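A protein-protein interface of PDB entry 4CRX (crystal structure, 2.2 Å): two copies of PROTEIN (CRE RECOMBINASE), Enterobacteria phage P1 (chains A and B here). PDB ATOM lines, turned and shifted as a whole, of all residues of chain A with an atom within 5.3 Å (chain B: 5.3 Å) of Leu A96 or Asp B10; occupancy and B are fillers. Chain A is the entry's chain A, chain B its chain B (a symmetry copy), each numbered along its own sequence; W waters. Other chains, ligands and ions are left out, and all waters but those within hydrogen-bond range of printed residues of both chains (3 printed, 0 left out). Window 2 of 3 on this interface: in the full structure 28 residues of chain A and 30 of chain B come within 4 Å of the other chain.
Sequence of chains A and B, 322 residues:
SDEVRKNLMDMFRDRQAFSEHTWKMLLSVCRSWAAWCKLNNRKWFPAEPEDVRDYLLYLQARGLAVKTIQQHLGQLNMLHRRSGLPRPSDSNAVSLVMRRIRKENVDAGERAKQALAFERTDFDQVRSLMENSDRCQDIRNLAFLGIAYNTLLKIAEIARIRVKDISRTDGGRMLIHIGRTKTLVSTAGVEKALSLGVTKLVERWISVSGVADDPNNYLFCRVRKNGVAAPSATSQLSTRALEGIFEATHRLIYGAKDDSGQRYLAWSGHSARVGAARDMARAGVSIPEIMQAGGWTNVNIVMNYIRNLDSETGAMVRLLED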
ATOM      1  N   GLU A  50      -1.851 -25.883  16.004  1.00  0.00           N
ATOM      2  CA  GLU A  50      -1.211 -25.852  14.692  1.00  0.00           C
ATOM      3  C   GLU A  50      -2.256 -25.623  13.598  1.00  0.00           C
ATOM      4  O   GLU A  50      -1.945 -25.075  12.539  1.00  0.00           O
ATOM      5  CB  GLU A  50      -0.442 -27.157  14.438  1.00  0.00           C
ATOM      6  CG  GLU A  50       0.977 -26.969  13.875  1.00  0.00           C
ATOM      7  CD  GLU A  50       1.981 -26.468  14.908  1.00  0.00           C
ATOM      8  OE1 GLU A  50       1.847 -26.806  16.102  1.00  0.00           O
ATOM      9  OE2 GLU A  50       2.913 -25.730  14.527  1.00  0.00           O
ATOM     10  N   SER A  91      -1.352 -21.108  23.393  1.00  0.00           N
ATOM     11  CA  SER A  91      -0.310 -21.952  22.820  1.00  0.00           C
ATOM     12  C   SER A  91       0.766 -21.057  22.192  1.00  0.00           C
ATOM     13  O   SER A  91       0.477 -19.948  21.740  1.00  0.00           O
ATOM     14  CB  SER A  91      -0.899 -22.912  21.777  1.00  0.00           C
ATOM     15  OG  SER A  91      -1.414 -22.215  20.660  1.00  0.00           O
ATOM     16  N   ASN A  92       2.007 -21.540  22.185  1.00  0.00           N
ATOM     17  CA  ASN A  92       3.142 -20.792  21.636  1.00  0.00           C
ATOM     18  C   ASN A  92       2.964 -20.445  20.158  1.00  0.00           C
ATOM     19  O   ASN A  92       3.152 -19.297  19.746  1.00  0.00           O
ATOM     20  CB  ASN A  92       4.443 -21.600  21.816  1.00  0.00           C
ATOM     21  CG  ASN A  92       5.698 -20.733  21.714  1.00  0.00           C
ATOM     22  OD1 ASN A  92       5.729 -19.619  22.229  1.00  0.00           O
ATOM     23  ND2 ASN A  92       6.738 -21.246  21.056  1.00  0.00           N
ATOM     24  N   ALA A  93       2.600 -21.450  19.368  1.00  0.00           N
ATOM     25  CA  ALA A  93       2.411 -21.291  17.929  1.00  0.00           C
ATOM     26  C   ALA A  93       1.409 -20.207  17.552  1.00  0.00           C
ATOM     27  O   ALA A  93       1.664 -19.397  16.662  1.00  0.00           O
ATOM     28  CB  ALA A  93       1.977 -22.622  17.324  1.00  0.00           C
ATOM     29  N   VAL A  94       0.265 -20.198  18.229  1.00  0.00           N
ATOM     30  CA  VAL A  94      -0.787 -19.222  17.947  1.00  0.00           C
ATOM     31  C   VAL A  94      -0.376 -17.820  18.392  1.00  0.00           C
ATOM     32  O   VAL A  94      -0.674 -16.825  17.726  1.00  0.00           O
ATOM     33  CB  VAL A  94      -2.116 -19.620  18.657  1.00  0.00           C
ATOM     34  CG1 VAL A  94      -3.157 -18.531  18.490  1.00  0.00           C
ATOM     35  CG2 VAL A  94      -2.659 -20.920  18.084  1.00  0.00           C
ATOM     36  N   SER A  95       0.313 -17.760  19.526  1.00  0.00           N
ATOM     37  CA  SER A  95       0.777 -16.504  20.108  1.00  0.00           C
ATOM     38  C   SER A  95       1.794 -15.817  19.206  1.00  0.00           C
ATOM     39  O   SER A  95       1.854 -14.586  19.130  1.00  0.00           O
ATOM     40  CB  SER A  95       1.404 -16.779  21.473  1.00  0.00           C
ATOM     41  OG  SER A  95       0.785 -16.002  22.482  1.00  0.00           O
ATOM     42  N   LEU A  96       2.594 -16.636  18.528  1.00  0.00           N
ATOM     43  CA  LEU A  96       3.629 -16.160  17.619  1.00  0.00           C
ATOM     44  C   LEU A  96       3.046 -15.630  16.307  1.00  0.00           C
ATOM     45  O   LEU A  96       3.451 -14.564  15.843  1.00  0.00           O
ATOM     46  CB  LEU A  96       4.644 -17.285  17.338  1.00  0.00           C
ATOM     47  CG  LEU A  96       5.618 -17.633  18.482  1.00  0.00           C
ATOM     48  CD1 LEU A  96       6.539 -18.774  18.087  1.00  0.00           C
ATOM     49  CD2 LEU A  96       6.465 -16.423  18.838  1.00  0.00           C
ATOM     50  N   VAL A  97       2.096 -16.359  15.712  1.00  0.00           N
ATOM     51  CA  VAL A  97       1.488 -15.928  14.441  1.00  0.00           C
ATOM     52  C   VAL A  97       0.679 -14.655  14.596  1.00  0.00           C
ATOM     53  O   VAL A  97       0.670 -13.806  13.707  1.00  0.00           O
ATOM     54  CB  VAL A  97       0.522 -16.980  13.812  1.00  0.00           C
ATOM     55  CG1 VAL A  97       1.184 -17.665  12.642  1.00  0.00           C
ATOM     56  CG2 VAL A  97       0.071 -17.991  14.828  1.00  0.00           C
ATOM     57  N   MET A  98      -0.028 -14.538  15.712  1.00  0.00           N
ATOM     58  CA  MET A  98      -0.838 -13.354  15.959  1.00  0.00           C
ATOM     59  C   MET A  98       0.082 -12.149  16.064  1.00  0.00           C
ATOM     60  O   MET A  98      -0.214 -11.074  15.545  1.00  0.00           O
ATOM     61  CB  MET A  98      -1.628 -13.516  17.258  1.00  0.00           C
ATOM     62  CG  MET A  98      -3.059 -13.986  17.060  1.00  0.00           C
ATOM     63  SD  MET A  98      -3.935 -13.108  15.730  1.00  0.00           S
ATOM     64  CE  MET A  98      -4.619 -11.662  16.543  1.00  0.00           C
ATOM     65  N   ARG A  99       1.206 -12.347  16.743  1.00  0.00           N
ATOM     66  CA  ARG A  99       2.198 -11.299  16.926  1.00  0.00           C
ATOM     67  C   ARG A  99       2.798 -10.920  15.577  1.00  0.00           C
ATOM     68  O   ARG A  99       2.965  -9.743  15.261  1.00  0.00           O
ATOM     69  CB  ARG A  99       3.302 -11.800  17.857  1.00  0.00           C
ATOM     70  CG  ARG A  99       4.021 -10.716  18.633  1.00  0.00           C
ATOM     71  CD  ARG A  99       5.513 -10.994  18.662  1.00  0.00           C
ATOM     72  NE  ARG A  99       6.257  -9.985  19.410  1.00  0.00           N
ATOM     73  CZ  ARG A  99       6.996 -10.249  20.484  1.00  0.00           C
ATOM     74  NH1 ARG A  99       7.086 -11.492  20.938  1.00  0.00           N
ATOM     75  NH2 ARG A  99       7.643  -9.273  21.105  1.00  0.00           N
ATOM     76  N   ARG A 100       3.110 -11.935  14.781  1.00  0.00           N
ATOM     77  CA  ARG A 100       3.707 -11.722  13.475  1.00  0.00           C
ATOM     78  C   ARG A 100       2.714 -11.168  12.458  1.00  0.00           C
ATOM     79  O   ARG A 100       3.077 -10.358  11.605  1.00  0.00           O
ATOM     80  CB  ARG A 100       4.318 -13.035  12.986  1.00  0.00           C
ATOM     81  CG  ARG A 100       3.728 -13.582  11.722  1.00  0.00           C
ATOM     82  CD  ARG A 100       4.663 -14.608  11.153  1.00  0.00           C
ATOM     83  NE  ARG A 100       4.450 -14.788   9.726  1.00  0.00           N
ATOM     84  CZ  ARG A 100       4.519 -15.962   9.113  1.00  0.00           C
ATOM     85  NH1 ARG A 100       4.795 -17.057   9.806  1.00  0.00           N
ATOM     86  NH2 ARG A 100       4.312 -16.039   7.807  1.00  0.00           N
ATOM     87  N   ILE A 101       1.460 -11.595  12.560  1.00  0.00           N
ATOM     88  CA  ILE A 101       0.415 -11.132  11.653  1.00  0.00           C
ATOM     89  C   ILE A 101       0.162  -9.653  11.936  1.00  0.00           C
ATOM     90  O   ILE A 101       0.056  -8.846  11.013  1.00  0.00           O
ATOM     91  CB  ILE A 101      -0.904 -11.934  11.860  1.00  0.00           C
ATOM     92  CG1 ILE A 101      -0.858 -13.247  11.076  1.00  0.00           C
ATOM     93  CG2 ILE A 101      -2.099 -11.120  11.388  1.00  0.00           C
ATOM     94  CD1 ILE A 101      -1.923 -14.241  11.500  1.00  0.00           C
ATOM     95  N   ARG B   5      14.005 -28.701  20.325  1.00  0.00           N
ATOM     96  CA  ARG B   5      14.167 -28.570  18.886  1.00  0.00           C
ATOM     97  C   ARG B   5      12.897 -27.986  18.273  1.00  0.00           C
ATOM     98  O   ARG B   5      12.957 -27.248  17.288  1.00  0.00           O
ATOM     99  CB  ARG B   5      14.462 -29.946  18.276  1.00  0.00           C
ATOM    100  CG  ARG B   5      15.870 -30.090  17.697  1.00  0.00           C
ATOM    101  CD  ARG B   5      16.866 -30.678  18.707  1.00  0.00           C
ATOM    102  NE  ARG B   5      18.151 -31.050  18.104  1.00  0.00           N
ATOM    103  CZ  ARG B   5      19.343 -30.751  18.620  1.00  0.00           C
ATOM    104  NH1 ARG B   5      19.425 -30.087  19.764  1.00  0.00           N
ATOM    105  NH2 ARG B   5      20.462 -31.128  18.008  1.00  0.00           N
ATOM    106  N   LYS B   6      11.751 -28.311  18.865  1.00  0.00           N
ATOM    107  CA  LYS B   6      10.465 -27.824  18.371  1.00  0.00           C
ATOM    108  C   LYS B   6      10.263 -26.341  18.638  1.00  0.00           C
ATOM    109  O   LYS B   6       9.937 -25.582  17.729  1.00  0.00           O
ATOM    110  CB  LYS B   6       9.311 -28.603  19.007  1.00  0.00           C
ATOM    111  CG  LYS B   6       8.018 -28.555  18.197  1.00  0.00           C
ATOM    112  CD  LYS B   6       6.890 -27.866  18.957  1.00  0.00           C
ATOM    113  CE  LYS B   6       5.626 -27.719  18.102  1.00  0.00           C
ATOM    114  NZ  LYS B   6       5.887 -27.538  16.639  1.00  0.00           N
ATOM    115  N   ASN B   7      10.443 -25.943  19.895  1.00  0.00           N
ATOM    116  CA  ASN B   7      10.288 -24.552  20.310  1.00  0.00           C
ATOM    117  C   ASN B   7      11.184 -23.649  19.499  1.00  0.00           C
ATOM    118  O   ASN B   7      10.807 -22.536  19.137  1.00  0.00           O
ATOM    119  CB  ASN B   7      10.658 -24.399  21.778  1.00  0.00           C
ATOM    120  CG  ASN B   7       9.840 -25.286  22.663  1.00  0.00           C
ATOM    121  OD1 ASN B   7       8.758 -25.726  22.278  1.00  0.00           O
ATOM    122  ND2 ASN B   7      10.343 -25.563  23.856  1.00  0.00           N
ATOM    123  N   LEU B   8      12.390 -24.128  19.236  1.00  0.00           N
ATOM    124  CA  LEU B   8      13.329 -23.349  18.463  1.00  0.00           C
ATOM    125  C   LEU B   8      12.805 -23.252  17.042  1.00  0.00           C
ATOM    126  O   LEU B   8      12.725 -22.164  16.480  1.00  0.00           O
ATOM    127  CB  LEU B   8      14.710 -24.004  18.483  1.00  0.00           C
ATOM    128  CG  LEU B   8      15.842 -23.247  19.188  1.00  0.00           C
ATOM    129  CD1 LEU B   8      15.315 -21.996  19.874  1.00  0.00           C
ATOM    130  CD2 LEU B   8      16.501 -24.168  20.197  1.00  0.00           C
ATOM    131  N   MET B   9      12.429 -24.391  16.471  1.00  0.00           N
ATOM    132  CA  MET B   9      11.912 -24.414  15.111  1.00  0.00           C
ATOM    133  C   MET B   9      10.671 -23.528  14.998  1.00  0.00           C
ATOM    134  O   MET B   9      10.447 -22.893  13.971  1.00  0.00           O
ATOM    135  CB  MET B   9      11.569 -25.850  14.698  1.00  0.00           C
ATOM    136  CG  MET B   9      12.771 -26.681  14.243  1.00  0.00           C
ATOM    137  SD  MET B   9      12.453 -28.471  14.263  1.00  0.00           S
ATOM    138  CE  MET B   9      13.790 -29.095  13.231  1.00  0.00           C
ATOM    139  N   ASP B  10       9.877 -23.481  16.064  1.00  0.00           N
ATOM    140  CA  ASP B  10       8.660 -22.677  16.082  1.00  0.00           C
ATOM    141  C   ASP B  10       8.990 -21.188  16.128  1.00  0.00           C
ATOM    142  O   ASP B  10       8.275 -20.365  15.551  1.00  0.00           O
ATOM    143  CB  ASP B  10       7.798 -23.034  17.299  1.00  0.00           C
ATOM    144  CG  ASP B  10       6.933 -24.261  17.069  1.00  0.00           C
ATOM    145  OD1 ASP B  10       6.963 -24.823  15.952  1.00  0.00           O
ATOM    146  OD2 ASP B  10       6.215 -24.672  18.009  1.00  0.00           O
ATOM    147  N   MET B  11      10.067 -20.844  16.827  1.00  0.00           N
ATOM    148  CA  MET B  11      10.474 -19.451  16.949  1.00  0.00           C
ATOM    149  C   MET B  11      10.968 -18.928  15.618  1.00  0.00           C
ATOM    150  O   MET B  11      10.663 -17.802  15.224  1.00  0.00           O
ATOM    151  CB  MET B  11      11.585 -19.298  17.986  1.00  0.00           C
ATOM    152  CG  MET B  11      11.722 -17.877  18.474  1.00  0.00           C
ATOM    153  SD  MET B  11      13.095 -17.557  19.612  1.00  0.00           S
ATOM    154  CE  MET B  11      14.346 -18.778  19.164  1.00  0.00           C
ATOM    155  N   PHE B  12      11.739 -19.758  14.928  1.00  0.00           N
ATOM    156  CA  PHE B  12      12.280 -19.383  13.635  1.00  0.00           C
ATOM    157  C   PHE B  12      11.181 -19.335  12.578  1.00  0.00           C
ATOM    158  O   PHE B  12      11.213 -18.505  11.671  1.00  0.00           O
ATOM    159  CB  PHE B  12      13.353 -20.378  13.204  1.00  0.00           C
ATOM    160  CG  PHE B  12      13.669 -20.303  11.743  1.00  0.00           C
ATOM    161  CD1 PHE B  12      14.325 -19.191  11.225  1.00  0.00           C
ATOM    162  CD2 PHE B  12      13.293 -21.328  10.883  1.00  0.00           C
ATOM    163  CE1 PHE B  12      14.582 -19.091   9.862  1.00  0.00           C
ATOM    164  CE2 PHE B  12      13.543 -21.238   9.516  1.00  0.00           C
ATOM    165  CZ  PHE B  12      14.198 -20.119   9.005  1.00  0.00           C
ATOM    166  N   ARG B  13      10.213 -20.238  12.698  1.00  0.00           N
ATOM    167  CA  ARG B  13       9.105 -20.296  11.752  1.00  0.00           C
ATOM    168  C   ARG B  13       8.365 -18.965  11.733  1.00  0.00           C
ATOM    169  O   ARG B  13       8.044 -18.434  10.666  1.00  0.00           O
ATOM    170  CB  ARG B  13       8.130 -21.406  12.138  1.00  0.00           C
ATOM    171  CG  ARG B  13       7.065 -21.668  11.086  1.00  0.00           C
ATOM    172  CD  ARG B  13       6.138 -22.821  11.465  1.00  0.00           C
ATOM    173  NE  ARG B  13       5.656 -22.748  12.843  1.00  0.00           N
ATOM    174  CZ  ARG B  13       4.804 -23.621  13.376  1.00  0.00           C
ATOM    175  NH1 ARG B  13       4.366 -24.638  12.649  1.00  0.00           N
ATOM    176  NH2 ARG B  13       4.399 -23.491  14.635  1.00  0.00           N
ATOM    177  N   ASP B  14       8.095 -18.449  12.932  1.00  0.00           N
ATOM    178  CA  ASP B  14       7.387 -17.184  13.119  1.00  0.00           C
ATOM    179  C   ASP B  14       8.353 -16.105  13.596  1.00  0.00           C
ATOM    180  O   ASP B  14       8.174 -15.481  14.649  1.00  0.00           O
ATOM    181  CB  ASP B  14       6.251 -17.358  14.133  1.00  0.00           C
ATOM    182  CG  ASP B  14       5.078 -18.133  13.567  1.00  0.00           C
ATOM    183  OD1 ASP B  14       4.744 -17.940  12.376  1.00  0.00           O
ATOM    184  OD2 ASP B  14       4.482 -18.940  14.312  1.00  0.00           O
ATOM    185  N   ALA B  17       7.558 -12.355  14.040  1.00  0.00           N
ATOM    186  CA  ALA B  17       6.857 -11.911  15.230  1.00  0.00           C
ATOM    187  C   ALA B  17       7.781 -10.907  15.896  1.00  0.00           C
ATOM    188  O   ALA B  17       7.352 -10.083  16.699  1.00  0.00           O
ATOM    189  CB  ALA B  17       6.605 -13.080  16.166  1.00  0.00           C
ATOM    190  N   PHE B  18       9.058 -10.985  15.537  1.00  0.00           N
ATOM    191  CA  PHE B  18      10.082 -10.118  16.101  1.00  0.00           C
ATOM    192  C   PHE B  18      10.659  -9.152  15.073  1.00  0.00           C
ATOM    193  O   PHE B  18      10.611  -9.407  13.869  1.00  0.00           O
ATOM    194  CB  PHE B  18      11.223 -10.964  16.682  1.00  0.00           C
ATOM    195  CG  PHE B  18      10.776 -11.982  17.695  1.00  0.00           C
ATOM    196  CD1 PHE B  18      10.685 -11.646  19.042  1.00  0.00           C
ATOM    197  CD2 PHE B  18      10.437 -13.274  17.304  1.00  0.00           C
ATOM    198  CE1 PHE B  18      10.265 -12.581  19.982  1.00  0.00           C
ATOM    199  CE2 PHE B  18      10.017 -14.216  18.238  1.00  0.00           C
ATOM    200  CZ  PHE B  18       9.928 -13.868  19.579  1.00  0.00           C
ATOM    201  N   ARG B  82      13.012 -19.033  25.249  1.00  0.00           N
ATOM    202  CA  ARG B  82      12.116 -19.330  24.138  1.00  0.00           C
ATOM    203  C   ARG B  82      12.263 -20.766  23.626  1.00  0.00           C
ATOM    204  O   ARG B  82      11.462 -21.231  22.817  1.00  0.00           O
ATOM    205  CB  ARG B  82      12.332 -18.310  23.011  1.00  0.00           C
ATOM    206  CG  ARG B  82      11.121 -17.376  22.805  1.00  0.00           C
ATOM    207  CD  ARG B  82      11.487 -15.904  22.558  1.00  0.00           C
ATOM    208  NE  ARG B  82      10.605 -14.938  23.240  1.00  0.00           N
ATOM    209  CZ  ARG B  82       9.272 -14.915  23.158  1.00  0.00           C
ATOM    210  NH1 ARG B  82       8.629 -15.821  22.440  1.00  0.00           N
ATOM    211  NH2 ARG B  82       8.567 -13.987  23.797  1.00  0.00           N
HETATM  212  O   HOH W   1       9.732 -20.702  20.796  1.00  0.00           O
HETATM  213  O   HOH W   2       8.273 -18.201  21.999  1.00  0.00           O
HETATM  214  O   HOH W   3       6.105 -24.471  20.805  1.00  0.00           O
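NH1 of Arg B13 is in salt-bridge range of OE2 of Glu A50. NE of Arg A99 lies close to O of Ala B17. The side-chain carboxylate (OD1) of Asp B14 is in salt-bridge range of the guanidinium group (NH1) of Arg A100, 2.7 Å away.
NZ of Lys B6 lies within salt-bridge range of OD1 of Asp B10 (3.0 Å). NH2 of Arg B13 lies within salt-bridge range of OD1 of Asp B10.
Among the printed residues, merely in contact across the chains: Ala A93 with Arg B13 (3.7 Å), Ala A93 with Asp B14 (3.7 Å), Leu A96 with Asp B10 (3.5 Å), Leu A96 with Asp B14 (3.5 Å), Leu A96 with Ala B17 (3.5 Å), Val A97 with Asp B14 (3.6 Å), Arg A99 with Phe B18 (3.5 Å), Arg A100 with Arg B13 (3.6 Å) and Arg A100 with Ala B17 (3.5 Å).
Of chain B, only Asp B10 (3.5 Å), Asp B14 (3.5 Å) and Ala B17 (3.5 Å) come within 4 Å of Leu A96. Of the printed residues of chain A, Asp B10 touches Leu A96. Of the printed residues of chain B, Arg A100 touches Arg B13 (3.6 Å), Asp B14 (2.7 Å) and Ala B17 (3.5 Å). Of the printed residues of chain B, Glu A50 touches Arg B13 (2.6 Å). Of the printed residues of chain A, Arg B13 touches Glu A50, Ala A93 and Arg A100. Of the printed residues of chain B, Val A97 touches Asp B14. The nearest printed residue of chain A that does not touch Asp B14 is Asn A92 (5.6 Å).
Of the 13 printed residues of chain B, 5 touch a printed residue of chain A. Printed residues of chain B that touch a printed residue of chain A: Asp B10, Arg B13, Asp B14, Ala B17 and Phe B18. Hydrophobic or aromatic side chains of chain B that line the printed part of chain A: Ala B17 and Phe B18. Of the 12 printed residues of chain A, 6 touch a printed residue of chain B. Among the printed residues, Asp or Glu carboxylates within 4 Å of a Lys or Arg side-chain nitrogen of the other chain: Glu A50 with Arg B13 (2.6 Å) and Arg A100 with Asp B14 (2.7 Å).
No position is printed for both chains.
Water W2 bridges the guanidinium group (NH1) of Arg B82 (2.4 Å) and the side-chain amide oxygen (OD1) of Asn A92 (2.9 Å). Water W1 lies within hydrogen-bond range of O of Asn B7 (2.7 Å), O of Arg B82 (2.7 Å) and ND2 of Asn A92 (3.1 Å). Water W3 lies within hydrogen-bond range of OD2 of Asp B10 (2.8 Å), OD1 of Asn B7 (3.3 Å) and ND2 of Asn A92 (3.3 Å).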
